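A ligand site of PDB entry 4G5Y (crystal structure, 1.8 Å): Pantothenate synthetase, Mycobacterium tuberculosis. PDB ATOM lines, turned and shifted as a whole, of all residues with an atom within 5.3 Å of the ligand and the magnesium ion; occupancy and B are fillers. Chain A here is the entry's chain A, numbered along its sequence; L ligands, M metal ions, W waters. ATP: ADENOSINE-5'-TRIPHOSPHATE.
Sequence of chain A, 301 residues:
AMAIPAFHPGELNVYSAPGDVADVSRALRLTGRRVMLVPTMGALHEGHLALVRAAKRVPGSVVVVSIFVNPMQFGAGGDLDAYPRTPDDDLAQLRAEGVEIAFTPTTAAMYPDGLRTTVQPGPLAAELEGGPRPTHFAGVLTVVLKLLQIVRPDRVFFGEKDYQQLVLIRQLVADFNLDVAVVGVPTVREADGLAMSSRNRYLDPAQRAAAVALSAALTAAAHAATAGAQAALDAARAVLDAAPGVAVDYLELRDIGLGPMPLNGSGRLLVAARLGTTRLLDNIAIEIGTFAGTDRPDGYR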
ATOM      1  N   PRO A  39      12.080  15.676 -28.192  1.00  0.00           N
ATOM      2  CA  PRO A  39      12.768  16.983 -28.368  1.00  0.00           C
ATOM      3  C   PRO A  39      14.242  16.876 -28.172  1.00  0.00           C
ATOM      4  O   PRO A  39      14.713  16.276 -27.127  1.00  0.00           O
ATOM      5  CB  PRO A  39      12.158  17.848 -27.322  1.00  0.00           C
ATOM      6  CG  PRO A  39      10.811  17.104 -26.910  1.00  0.00           C
ATOM      7  CD  PRO A  39      11.282  15.681 -26.965  1.00  0.00           C
ATOM      8  N   THR A  40      14.992  17.487 -29.113  1.00  0.00           N
ATOM      9  CA  THR A  40      16.477  17.468 -28.960  1.00  0.00           C
ATOM     10  C   THR A  40      17.038  18.871 -29.260  1.00  0.00           C
ATOM     11  O   THR A  40      16.361  19.744 -29.852  1.00  0.00           O
ATOM     12  CB  THR A  40      17.167  16.440 -29.910  1.00  0.00           C
ATOM     13  OG1 THR A  40      17.257  16.992 -31.248  1.00  0.00           O
ATOM     14  CG2 THR A  40      16.307  15.137 -29.971  1.00  0.00           C
ATOM     15  N   MET A  41      18.326  19.027 -28.895  1.00  0.00           N
ATOM     16  CA  MET A  41      19.094  20.221 -29.379  1.00  0.00           C
ATOM     17  C   MET A  41      20.068  19.825 -30.501  1.00  0.00           C
ATOM     18  O   MET A  41      21.099  20.459 -30.693  1.00  0.00           O
ATOM     19  CB  MET A  41      19.802  20.805 -28.118  1.00  0.00           C
ATOM     20  CG  MET A  41      18.812  21.457 -27.222  1.00  0.00           C
ATOM     21  SD  MET A  41      19.644  22.523 -25.987  1.00  0.00           S
ATOM     22  CE  MET A  41      20.788  21.339 -25.399  1.00  0.00           C
ATOM     23  N   GLY A  42      19.778  18.723 -31.200  1.00  0.00           N
ATOM     24  CA  GLY A  42      20.649  18.152 -32.248  1.00  0.00           C
ATOM     25  C   GLY A  42      21.954  17.599 -31.645  1.00  0.00           C
ATOM     26  O   GLY A  42      22.031  17.318 -30.413  1.00  0.00           O
ATOM     27  N   HIS A  45      23.474  11.623 -30.494  1.00  0.00           N
ATOM     28  CA  HIS A  45      24.237  10.389 -30.228  1.00  0.00           C
ATOM     29  C   HIS A  45      23.340   9.221 -29.779  1.00  0.00           C
ATOM     30  O   HIS A  45      22.123   9.332 -29.746  1.00  0.00           O
ATOM     31  CB  HIS A  45      25.296  10.740 -29.187  1.00  0.00           C
ATOM     32  CG  HIS A  45      24.706  11.356 -27.935  1.00  0.00           C
ATOM     33  ND1 HIS A  45      24.006  10.634 -27.065  1.00  0.00           N
ATOM     34  CD2 HIS A  45      24.658  12.676 -27.478  1.00  0.00           C
ATOM     35  CE1 HIS A  45      23.522  11.427 -26.060  1.00  0.00           C
ATOM     36  NE2 HIS A  45      23.975  12.677 -26.278  1.00  0.00           N
ATOM     37  N   GLY A  47      22.413   8.069 -27.037  1.00  0.00           N
ATOM     38  CA  GLY A  47      21.442   8.446 -25.989  1.00  0.00           C
ATOM     39  C   GLY A  47      20.157   8.990 -26.659  1.00  0.00           C
ATOM     40  O   GLY A  47      19.008   8.525 -26.352  1.00  0.00           O
ATOM     41  N   HIS A  48      20.320   9.918 -27.594  1.00  0.00           N
ATOM     42  CA  HIS A  48      19.110  10.404 -28.327  1.00  0.00           C
ATOM     43  C   HIS A  48      18.447   9.242 -29.062  1.00  0.00           C
ATOM     44  O   HIS A  48      17.210   9.168 -29.148  1.00  0.00           O
ATOM     45  CB  HIS A  48      19.466  11.448 -29.305  1.00  0.00           C
ATOM     46  CG  HIS A  48      20.155  12.626 -28.691  1.00  0.00           C
ATOM     47  ND1 HIS A  48      21.441  12.864 -28.907  1.00  0.00           N
ATOM     48  CD2 HIS A  48      19.682  13.652 -27.877  1.00  0.00           C
ATOM     49  CE1 HIS A  48      21.804  14.010 -28.277  1.00  0.00           C
ATOM     50  NE2 HIS A  48      20.726  14.477 -27.617  1.00  0.00           N
ATOM     51  N   LEU A  51      15.897   7.305 -27.155  1.00  0.00           N
ATOM     52  CA  LEU A  51      14.591   7.971 -27.144  1.00  0.00           C
ATOM     53  C   LEU A  51      13.834   7.676 -28.407  1.00  0.00           C
ATOM     54  O   LEU A  51      12.656   7.274 -28.355  1.00  0.00           O
ATOM     55  CB  LEU A  51      14.766   9.496 -27.015  1.00  0.00           C
ATOM     56  CG  LEU A  51      15.545  10.030 -25.820  1.00  0.00           C
ATOM     57  CD1 LEU A  51      15.137  11.493 -25.577  1.00  0.00           C
ATOM     58  CD2 LEU A  51      15.247   9.307 -24.562  1.00  0.00           C
ATOM     59  N   TYR A  83      27.351  25.805 -28.383  1.00  0.00           N
ATOM     60  CA  TYR A  83      26.649  24.549 -28.542  1.00  0.00           C
ATOM     61  C   TYR A  83      27.011  23.758 -29.849  1.00  0.00           C
ATOM     62  O   TYR A  83      26.941  24.343 -30.931  1.00  0.00           O
ATOM     63  CB  TYR A  83      25.114  24.736 -28.333  1.00  0.00           C
ATOM     64  CG  TYR A  83      24.554  23.410 -27.971  1.00  0.00           C
ATOM     65  CD1 TYR A  83      24.636  22.934 -26.651  1.00  0.00           C
ATOM     66  CD2 TYR A  83      24.060  22.556 -28.976  1.00  0.00           C
ATOM     67  CE1 TYR A  83      24.188  21.656 -26.332  1.00  0.00           C
ATOM     68  CE2 TYR A  83      23.606  21.295 -28.670  1.00  0.00           C
ATOM     69  CZ  TYR A  83      23.691  20.832 -27.350  1.00  0.00           C
ATOM     70  OH  TYR A  83      23.279  19.575 -27.027  1.00  0.00           O
ATOM     71  N   PRO A  84      27.414  22.445 -29.754  1.00  0.00           N
ATOM     72  CA  PRO A  84      27.717  21.643 -30.988  1.00  0.00           C
ATOM     73  C   PRO A  84      26.563  21.671 -32.002  1.00  0.00           C
ATOM     74  O   PRO A  84      25.410  21.293 -31.667  1.00  0.00           O
ATOM     75  CB  PRO A  84      27.901  20.187 -30.479  1.00  0.00           C
ATOM     76  CG  PRO A  84      27.526  20.185 -29.006  1.00  0.00           C
ATOM     77  CD  PRO A  84      27.579  21.626 -28.523  1.00  0.00           C
ATOM     78  N   PHE A 157       9.160  12.208 -25.137  1.00  0.00           N
ATOM     79  CA  PHE A 157      10.220  11.331 -24.589  1.00  0.00           C
ATOM     80  C   PHE A 157      11.397  12.193 -24.122  1.00  0.00           C
ATOM     81  O   PHE A 157      11.864  13.025 -24.900  1.00  0.00           O
ATOM     82  CB  PHE A 157      10.711  10.354 -25.724  1.00  0.00           C
ATOM     83  CG  PHE A 157       9.620   9.326 -26.070  1.00  0.00           C
ATOM     84  CD1 PHE A 157       8.536   9.708 -26.919  1.00  0.00           C
ATOM     85  CD2 PHE A 157       9.635   8.060 -25.479  1.00  0.00           C
ATOM     86  CE1 PHE A 157       7.498   8.765 -27.193  1.00  0.00           C
ATOM     87  CE2 PHE A 157       8.618   7.100 -25.808  1.00  0.00           C
ATOM     88  CZ  PHE A 157       7.570   7.508 -26.632  1.00  0.00           C
ATOM     89  N   PHE A 158      11.823  11.980 -22.864  1.00  0.00           N
ATOM     90  CA  PHE A 158      13.008  12.646 -22.318  1.00  0.00           C
ATOM     91  C   PHE A 158      13.916  11.631 -21.632  1.00  0.00           C
ATOM     92  O   PHE A 158      13.432  10.648 -21.071  1.00  0.00           O
ATOM     93  CB  PHE A 158      12.536  13.689 -21.277  1.00  0.00           C
ATOM     94  CG  PHE A 158      11.850  14.873 -21.910  1.00  0.00           C
ATOM     95  CD1 PHE A 158      12.576  15.919 -22.426  1.00  0.00           C
ATOM     96  CD2 PHE A 158      10.476  14.893 -22.027  1.00  0.00           C
ATOM     97  CE1 PHE A 158      11.915  17.024 -23.056  1.00  0.00           C
ATOM     98  CE2 PHE A 158       9.823  15.981 -22.652  1.00  0.00           C
ATOM     99  CZ  PHE A 158      10.546  17.041 -23.148  1.00  0.00           C
ATOM    100  N   GLY A 159      15.238  11.939 -21.543  1.00  0.00           N
ATOM    101  CA  GLY A 159      16.129  10.968 -20.921  1.00  0.00           C
ATOM    102  C   GLY A 159      16.153  11.173 -19.398  1.00  0.00           C
ATOM    103  O   GLY A 159      16.028  12.291 -18.887  1.00  0.00           O
ATOM    104  N   GLU A 160      16.373  10.104 -18.664  1.00  0.00           N
ATOM    105  CA  GLU A 160      16.594  10.199 -17.205  1.00  0.00           C
ATOM    106  C   GLU A 160      17.869  10.935 -16.875  1.00  0.00           C
ATOM    107  O   GLU A 160      18.048  11.389 -15.810  1.00  0.00           O
ATOM    108  CB  GLU A 160      16.706   8.827 -16.589  1.00  0.00           C
ATOM    109  CG  GLU A 160      15.303   8.243 -16.589  1.00  0.00           C
ATOM    110  CD  GLU A 160      15.136   6.920 -15.887  1.00  0.00           C
ATOM    111  OE1 GLU A 160      16.104   6.359 -15.372  1.00  0.00           O
ATOM    112  OE2 GLU A 160      14.027   6.384 -15.950  1.00  0.00           O
ATOM    113  N   LYS A 161      18.807  10.955 -17.826  1.00  0.00           N
ATOM    114  CA  LYS A 161      20.077  11.601 -17.558  1.00  0.00           C
ATOM    115  C   LYS A 161      19.884  13.030 -16.972  1.00  0.00           C
ATOM    116  O   LYS A 161      20.548  13.473 -16.006  1.00  0.00           O
ATOM    117  CB  LYS A 161      20.897  11.682 -18.856  1.00  0.00           C
ATOM    118  CG  LYS A 161      22.347  11.969 -18.418  1.00  0.00           C
ATOM    119  CD  LYS A 161      23.144  12.988 -19.164  1.00  0.00           C
ATOM    120  CE  LYS A 161      22.985  12.887 -20.640  1.00  0.00           C
ATOM    121  NZ  LYS A 161      23.145  14.248 -21.195  1.00  0.00           N
ATOM    122  N   ASP A 162      19.006  13.810 -17.634  1.00  0.00           N
ATOM    123  CA  ASP A 162      18.648  15.133 -17.156  1.00  0.00           C
ATOM    124  C   ASP A 162      17.398  14.947 -16.318  1.00  0.00           C
ATOM    125  O   ASP A 162      16.285  15.312 -16.711  1.00  0.00           O
ATOM    126  CB  ASP A 162      18.387  16.005 -18.387  1.00  0.00           C
ATOM    127  CG  ASP A 162      19.639  16.160 -19.212  1.00  0.00           C
ATOM    128  OD1 ASP A 162      20.504  16.907 -18.719  1.00  0.00           O
ATOM    129  OD2 ASP A 162      19.788  15.488 -20.268  1.00  0.00           O
ATOM    130  N   GLN A 165      15.339  18.015 -15.138  1.00  0.00           N
ATOM    131  CA  GLN A 165      14.552  18.508 -16.290  1.00  0.00           C
ATOM    132  C   GLN A 165      13.302  17.599 -16.492  1.00  0.00           C
ATOM    133  O   GLN A 165      12.212  18.110 -16.741  1.00  0.00           O
ATOM    134  CB  GLN A 165      15.446  18.407 -17.504  1.00  0.00           C
ATOM    135  CG  GLN A 165      14.662  18.579 -18.803  1.00  0.00           C
ATOM    136  CD  GLN A 165      15.577  18.755 -19.989  1.00  0.00           C
ATOM    137  OE1 GLN A 165      16.137  19.846 -20.186  1.00  0.00           O
ATOM    138  NE2 GLN A 165      15.813  17.680 -20.727  1.00  0.00           N
ATOM    139  N   VAL A 185      13.217   7.858 -20.370  1.00  0.00           N
ATOM    140  CA  VAL A 185      13.981   6.763 -20.948  1.00  0.00           C
ATOM    141  C   VAL A 185      15.306   6.626 -20.194  1.00  0.00           C
ATOM    142  O   VAL A 185      15.977   7.609 -19.948  1.00  0.00           O
ATOM    143  CB  VAL A 185      14.261   7.071 -22.400  1.00  0.00           C
ATOM    144  CG1 VAL A 185      15.117   5.959 -23.090  1.00  0.00           C
ATOM    145  CG2 VAL A 185      12.934   7.256 -23.103  1.00  0.00           C
ATOM    146  N   PRO A 186      15.691   5.391 -19.827  1.00  0.00           N
ATOM    147  CA  PRO A 186      16.897   5.210 -19.045  1.00  0.00           C
ATOM    148  C   PRO A 186      18.144   5.718 -19.770  1.00  0.00           C
ATOM    149  O   PRO A 186      18.256   5.644 -20.959  1.00  0.00           O
ATOM    150  CB  PRO A 186      16.994   3.685 -18.906  1.00  0.00           C
ATOM    151  CG  PRO A 186      15.559   3.247 -18.906  1.00  0.00           C
ATOM    152  CD  PRO A 186      14.978   4.102 -20.000  1.00  0.00           C
ATOM    153  N   THR A 187      19.067   6.216 -18.979  1.00  0.00           N
ATOM    154  CA  THR A 187      20.336   6.793 -19.459  1.00  0.00           C
ATOM    155  C   THR A 187      21.209   5.746 -20.200  1.00  0.00           C
ATOM    156  O   THR A 187      21.410   4.622 -19.710  1.00  0.00           O
ATOM    157  CB  THR A 187      21.049   7.349 -18.227  1.00  0.00           C
ATOM    158  OG1 THR A 187      20.252   8.445 -17.663  1.00  0.00           O
ATOM    159  CG2 THR A 187      22.474   7.843 -18.550  1.00  0.00           C
ATOM    160  N   VAL A 188      21.648   6.096 -21.390  1.00  0.00           N
ATOM    161  CA  VAL A 188      22.475   5.239 -22.204  1.00  0.00           C
ATOM    162  C   VAL A 188      23.915   5.598 -21.828  1.00  0.00           C
ATOM    163  O   VAL A 188      24.236   6.781 -21.696  1.00  0.00           O
ATOM    164  CB  VAL A 188      22.221   5.492 -23.738  1.00  0.00           C
ATOM    165  CG1 VAL A 188      23.239   4.666 -24.515  1.00  0.00           C
ATOM    166  CG2 VAL A 188      20.780   5.139 -24.092  1.00  0.00           C
ATOM    167  N   ARG A 189      24.777   4.580 -21.694  1.00  0.00           N
ATOM    168  CA  ARG A 189      26.107   4.802 -21.129  1.00  0.00           C
ATOM    169  C   ARG A 189      27.146   4.153 -22.026  1.00  0.00           C
ATOM    170  O   ARG A 189      26.843   3.214 -22.706  1.00  0.00           O
ATOM    171  CB  ARG A 189      26.148   4.129 -19.763  1.00  0.00           C
ATOM    172  CG  ARG A 189      25.228   4.845 -18.732  1.00  0.00           C
ATOM    173  CD  ARG A 189      25.248   4.092 -17.402  1.00  0.00           C
ATOM    174  NE  ARG A 189      24.383   4.811 -16.424  1.00  0.00           N
ATOM    175  CZ  ARG A 189      24.652   5.939 -15.844  1.00  0.00           C
ATOM    176  NH1 ARG A 189      25.857   6.492 -15.991  1.00  0.00           N
ATOM    177  NH2 ARG A 189      23.694   6.514 -15.029  1.00  0.00           N
ATOM    178  N   ALA A 195      27.866   8.395 -18.768  1.00  0.00           N
ATOM    179  CA  ALA A 195      26.571   8.752 -19.423  1.00  0.00           C
ATOM    180  C   ALA A 195      26.821   9.426 -20.764  1.00  0.00           C
ATOM    181  O   ALA A 195      27.653  10.305 -20.824  1.00  0.00           O
ATOM    182  CB  ALA A 195      25.814   9.699 -18.552  1.00  0.00           C
ATOM    183  N   MET A 196      26.211   8.976 -21.859  1.00  0.00           N
ATOM    184  CA  MET A 196      26.414   9.643 -23.133  1.00  0.00           C
ATOM    185  C   MET A 196      25.941  11.097 -23.091  1.00  0.00           C
ATOM    186  O   MET A 196      24.914  11.424 -22.489  1.00  0.00           O
ATOM    187  CB  MET A 196      25.682   8.837 -24.219  1.00  0.00           C
ATOM    188  CG  MET A 196      26.593   7.595 -24.478  1.00  0.00           C
ATOM    189  SD  MET A 196      26.250   6.799 -26.030  1.00  0.00           S
ATOM    190  CE  MET A 196      27.221   7.975 -26.970  1.00  0.00           C
ATOM    191  N   SER A 197      26.705  12.009 -23.737  1.00  0.00           N
ATOM    192  CA  SER A 197      26.288  13.411 -23.658  1.00  0.00           C
ATOM    193  C   SER A 197      27.033  14.112 -24.769  1.00  0.00           C
ATOM    194  O   SER A 197      28.196  13.756 -25.029  1.00  0.00           O
ATOM    195  CB  SER A 197      26.726  14.035 -22.318  1.00  0.00           C
ATOM    196  OG  SER A 197      25.839  15.060 -21.919  1.00  0.00           O
ATOM    197  N   SER A 198      26.363  15.061 -25.438  1.00  0.00           N
ATOM    198  CA  SER A 198      27.069  15.807 -26.524  1.00  0.00           C
ATOM    199  C   SER A 198      28.263  16.517 -25.879  1.00  0.00           C
ATOM    200  O   SER A 198      29.284  16.704 -26.520  1.00  0.00           O
ATOM    201  CB  SER A 198      26.130  16.801 -27.222  1.00  0.00           C
ATOM    202  OG  SER A 198      25.104  16.026 -27.837  1.00  0.00           O
ATOM    203  N   ARG A 199      28.155  16.854 -24.593  1.00  0.00           N
ATOM    204  CA  ARG A 199      29.302  17.577 -23.979  1.00  0.00           C
ATOM    205  C   ARG A 199      30.567  16.711 -23.747  1.00  0.00           C
ATOM    206  O   ARG A 199      31.662  17.257 -23.538  1.00  0.00           O
ATOM    207  CB  ARG A 199      28.925  18.271 -22.695  1.00  0.00           C
ATOM    208  CG  ARG A 199      28.627  17.330 -21.589  1.00  0.00           C
ATOM    209  CD  ARG A 199      27.976  18.145 -20.514  1.00  0.00           C
ATOM    210  NE  ARG A 199      26.816  18.862 -21.020  1.00  0.00           N
ATOM    211  CZ  ARG A 199      26.013  19.576 -20.222  1.00  0.00           C
ATOM    212  NH1 ARG A 199      26.286  19.688 -18.926  1.00  0.00           N
ATOM    213  NH2 ARG A 199      24.945  20.182 -20.717  1.00  0.00           N
ATOM    214  N   ASN A 200      30.422  15.389 -23.840  1.00  0.00           N
ATOM    215  CA  ASN A 200      31.558  14.502 -23.596  1.00  0.00           C
ATOM    216  C   ASN A 200      32.630  14.786 -24.656  1.00  0.00           C
ATOM    217  O   ASN A 200      33.721  14.281 -24.516  1.00  0.00           O
ATOM    218  CB  ASN A 200      31.234  13.014 -23.725  1.00  0.00           C
ATOM    219  CG  ASN A 200      30.372  12.541 -22.534  1.00  0.00           C
ATOM    220  OD1 ASN A 200      30.199  13.306 -21.601  1.00  0.00           O
ATOM    221  ND2 ASN A 200      29.816  11.331 -22.600  1.00  0.00           N
HETATM  222  PG  ATP L   1      24.562  18.226 -23.827  1.00  0.00           P
HETATM  223  O1G ATP L   1      25.623  17.189 -23.433  1.00  0.00           O
HETATM  224  O2G ATP L   1      25.037  19.353 -24.736  1.00  0.00           O
HETATM  225  O3G ATP L   1      23.733  18.684 -22.635  1.00  0.00           O
HETATM  226  PB  ATP L   1      22.774  16.157 -24.449  1.00  0.00           P
HETATM  227  O1B ATP L   1      23.502  14.962 -24.896  1.00  0.00           O
HETATM  228  O2B ATP L   1      22.255  16.229 -23.020  1.00  0.00           O
HETATM  229  O3B ATP L   1      23.658  17.430 -24.877  1.00  0.00           O
HETATM  230  PA  ATP L   1      20.176  17.307 -25.566  1.00  0.00           P
HETATM  231  O1A ATP L   1      20.532  18.269 -24.452  1.00  0.00           O
HETATM  232  O2A ATP L   1      19.887  17.485 -27.046  1.00  0.00           O
HETATM  233  O3A ATP L   1      21.498  16.305 -25.510  1.00  0.00           O
HETATM  234  O5' ATP L   1      19.079  16.241 -25.032  1.00  0.00           O
HETATM  235  C5' ATP L   1      17.950  15.783 -25.782  1.00  0.00           C
HETATM  236  C4' ATP L   1      17.253  14.705 -24.937  1.00  0.00           C
HETATM  237  O4' ATP L   1      18.159  13.587 -24.909  1.00  0.00           O
HETATM  238  C3' ATP L   1      17.022  15.056 -23.487  1.00  0.00           C
HETATM  239  O3' ATP L   1      15.768  14.426 -23.183  1.00  0.00           O
HETATM  240  C2' ATP L   1      18.116  14.305 -22.723  1.00  0.00           C
HETATM  241  O2' ATP L   1      17.801  13.843 -21.377  1.00  0.00           O
HETATM  242  C1' ATP L   1      18.287  13.100 -23.591  1.00  0.00           C
HETATM  243  N9  ATP L   1      19.565  12.421 -23.385  1.00  0.00           N
HETATM  244  C8  ATP L   1      20.798  13.008 -23.467  1.00  0.00           C
HETATM  245  N7  ATP L   1      21.780  12.112 -23.169  1.00  0.00           N
HETATM  246  C5  ATP L   1      21.153  10.917 -22.918  1.00  0.00           C
HETATM  247  C6  ATP L   1      21.553   9.574 -22.507  1.00  0.00           C
HETATM  248  N6  ATP L   1      22.857   9.359 -22.367  1.00  0.00           N
HETATM  249  N1  ATP L   1      20.597   8.616 -22.321  1.00  0.00           N
HETATM  250  C2  ATP L   1      19.273   8.902 -22.463  1.00  0.00           C
HETATM  251  N3  ATP L   1      18.844  10.146 -22.794  1.00  0.00           N
HETATM  252  C4  ATP L   1      19.698  11.147 -23.047  1.00  0.00           C
HETATM  253 MG    MG M   1      21.686  18.033 -22.003  1.00  0.00          MG
HETATM  254  O   HOH W   1      17.482  18.510 -23.127  1.00  0.00           O
HETATM  255  O   HOH W   2      15.247  14.852 -19.358  1.00  0.00           O
HETATM  256  O   HOH W   3      21.566  20.021 -23.078  1.00  0.00           O
HETATM  257  O   HOH W   4      22.371  17.404 -20.430  1.00  0.00           O
HETATM  258  O   HOH W   5      27.143  20.410 -25.581  1.00  0.00           O
HETATM  259  O   HOH W   6      14.101  14.667 -25.164  1.00  0.00           O
HETATM  260  O   HOH W   7      19.725  17.704 -21.645  1.00  0.00           O
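OG of Ser 197 sits at hydrogen-bond distance from NZ of Lys 161, at 2.9 Å. The side-chain amide nitrogen (ND2) of Asn 200 sits close to the backbone NH (N) of Ser 197, at 3.4 Å. The backbone NH of His 45 is in hydrogen-bond range of a ring nitrogen (ND1) of His 48, at 2.9 Å. A ring nitrogen (NE2) of His 45 sits at hydrogen-bond distance from the backbone NH (N) of Ser 198 (3.5 Å). OD2 of Asp 162 lies within salt-bridge range of NZ of Lys 161 (3.7 Å). The backbone carbonyl oxygen (O) of Val 188 sits at hydrogen-bond distance from the backbone NH (N) of Met 196, at 3.0 Å. The backbone carbonyl oxygen of Phe 158 sits at hydrogen-bond distance from the backbone NH of Val 185 (2.9 Å). OG1 of Thr 40 lies within hydrogen-bond range of N of Gly 42 (3.1 Å).
Asp 162 touches the magnesium ion.
Water W7 lies within hydrogen-bond range of the side-chain carboxylate (OD2) of Asp 162 and an oxygen (O1A) of the ligand. Water W4 lies within hydrogen-bond range of OD1 of Asp 162 and NZ of Lys 161. Water W6 lies within hydrogen-bond range of an oxygen (O3') of the ligand (2.6 Å), the backbone carbonyl oxygen of Pro 39 (2.6 Å) and the backbone carbonyl oxygen of Phe 157 (2.8 Å). Water W1 bridges the side-chain amide nitrogen (NE2) of Gln 165 and an oxygen (O1A) of the ligand. Water W2 lies within hydrogen-bond range of the backbone carbonyl oxygen of Gly 159 (2.7 Å), the backbone carbonyl oxygen of Asp 162 (2.9 Å), the side-chain amide nitrogen of Gln 165 (3.2 Å) and an oxygen (O2') of the ligand (3.4 Å).
O1G of the ligand lies within hydrogen-bond range of OG of Ser 197 (2.6 Å). A ring nitrogen (NE2) of His 45 lies within hydrogen-bond range of an oxygen (O1B) of the ligand (2.7 Å). The backbone NH (N) of Arg 199 lies within hydrogen-bond range of an oxygen (O1G) of the ligand. NE of Arg 199 is in salt-bridge range of O1G of the ligand, 3.2 Å away. The side-chain carboxylate (OD2) of Asp 162 lies within hydrogen-bond range of an oxygen (O2') of the ligand. NZ of Lys 161 is in salt-bridge range of O1B of the ligand. The backbone NH (N) of Met 41 is in hydrogen-bond range of an oxygen (O2A) of the ligand, at 2.9 Å. N of Val 188 is in hydrogen-bond range of N1 of the ligand. The backbone carbonyl oxygen of Val 188 sits at hydrogen-bond distance from a nitrogen (N6) of the ligand, at 3.0 Å. NE2 of His 48 is in hydrogen-bond range of O3A of the ligand (2.9 Å). O2G of the ligand sits at hydrogen-bond distance from OH of Tyr 83 (2.9 Å). The backbone NH of Ser 198 sits at hydrogen-bond distance from an oxygen (O1B) of the ligand, at 2.9 Å. The backbone carbonyl oxygen (O) of Met 196 lies within hydrogen-bond range of a nitrogen (N6) of the ligand (2.9 Å). N of Gly 159 sits at hydrogen-bond distance from O3' of the ligand (3.0 Å). The backbone carbonyl oxygen (O) of Gly 159 sits close to an oxygen (O2') of the ligand (3.4 Å).
Merely in contact with the ligand: Phe 158 (3.4 Å), Thr 187 (3.4 Å), Pro 39 (3.5 Å), Gly 47 (3.7 Å), Pro 186 (3.7 Å), Leu 51 (3.7 Å), Thr 40 (3.9 Å), Gly 42 (3.995 Å) and Gln 165 (3.996 Å). Hydrophobic or aromatic side chains that line the ligand: Met 41, His 45, His 48, Leu 51, Tyr 83, Phe 158, Val 188 and Met 196.
The magnesium ion is bound by water W4 (1.8 Å), water W7 (2.0 Å), O2B of the ligand (2.1 Å), O3G of the ligand (2.2 Å) and water W3 (2.3 Å). Slightly farther from the magnesium ion lies O1A of the ligand (2.7 Å).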
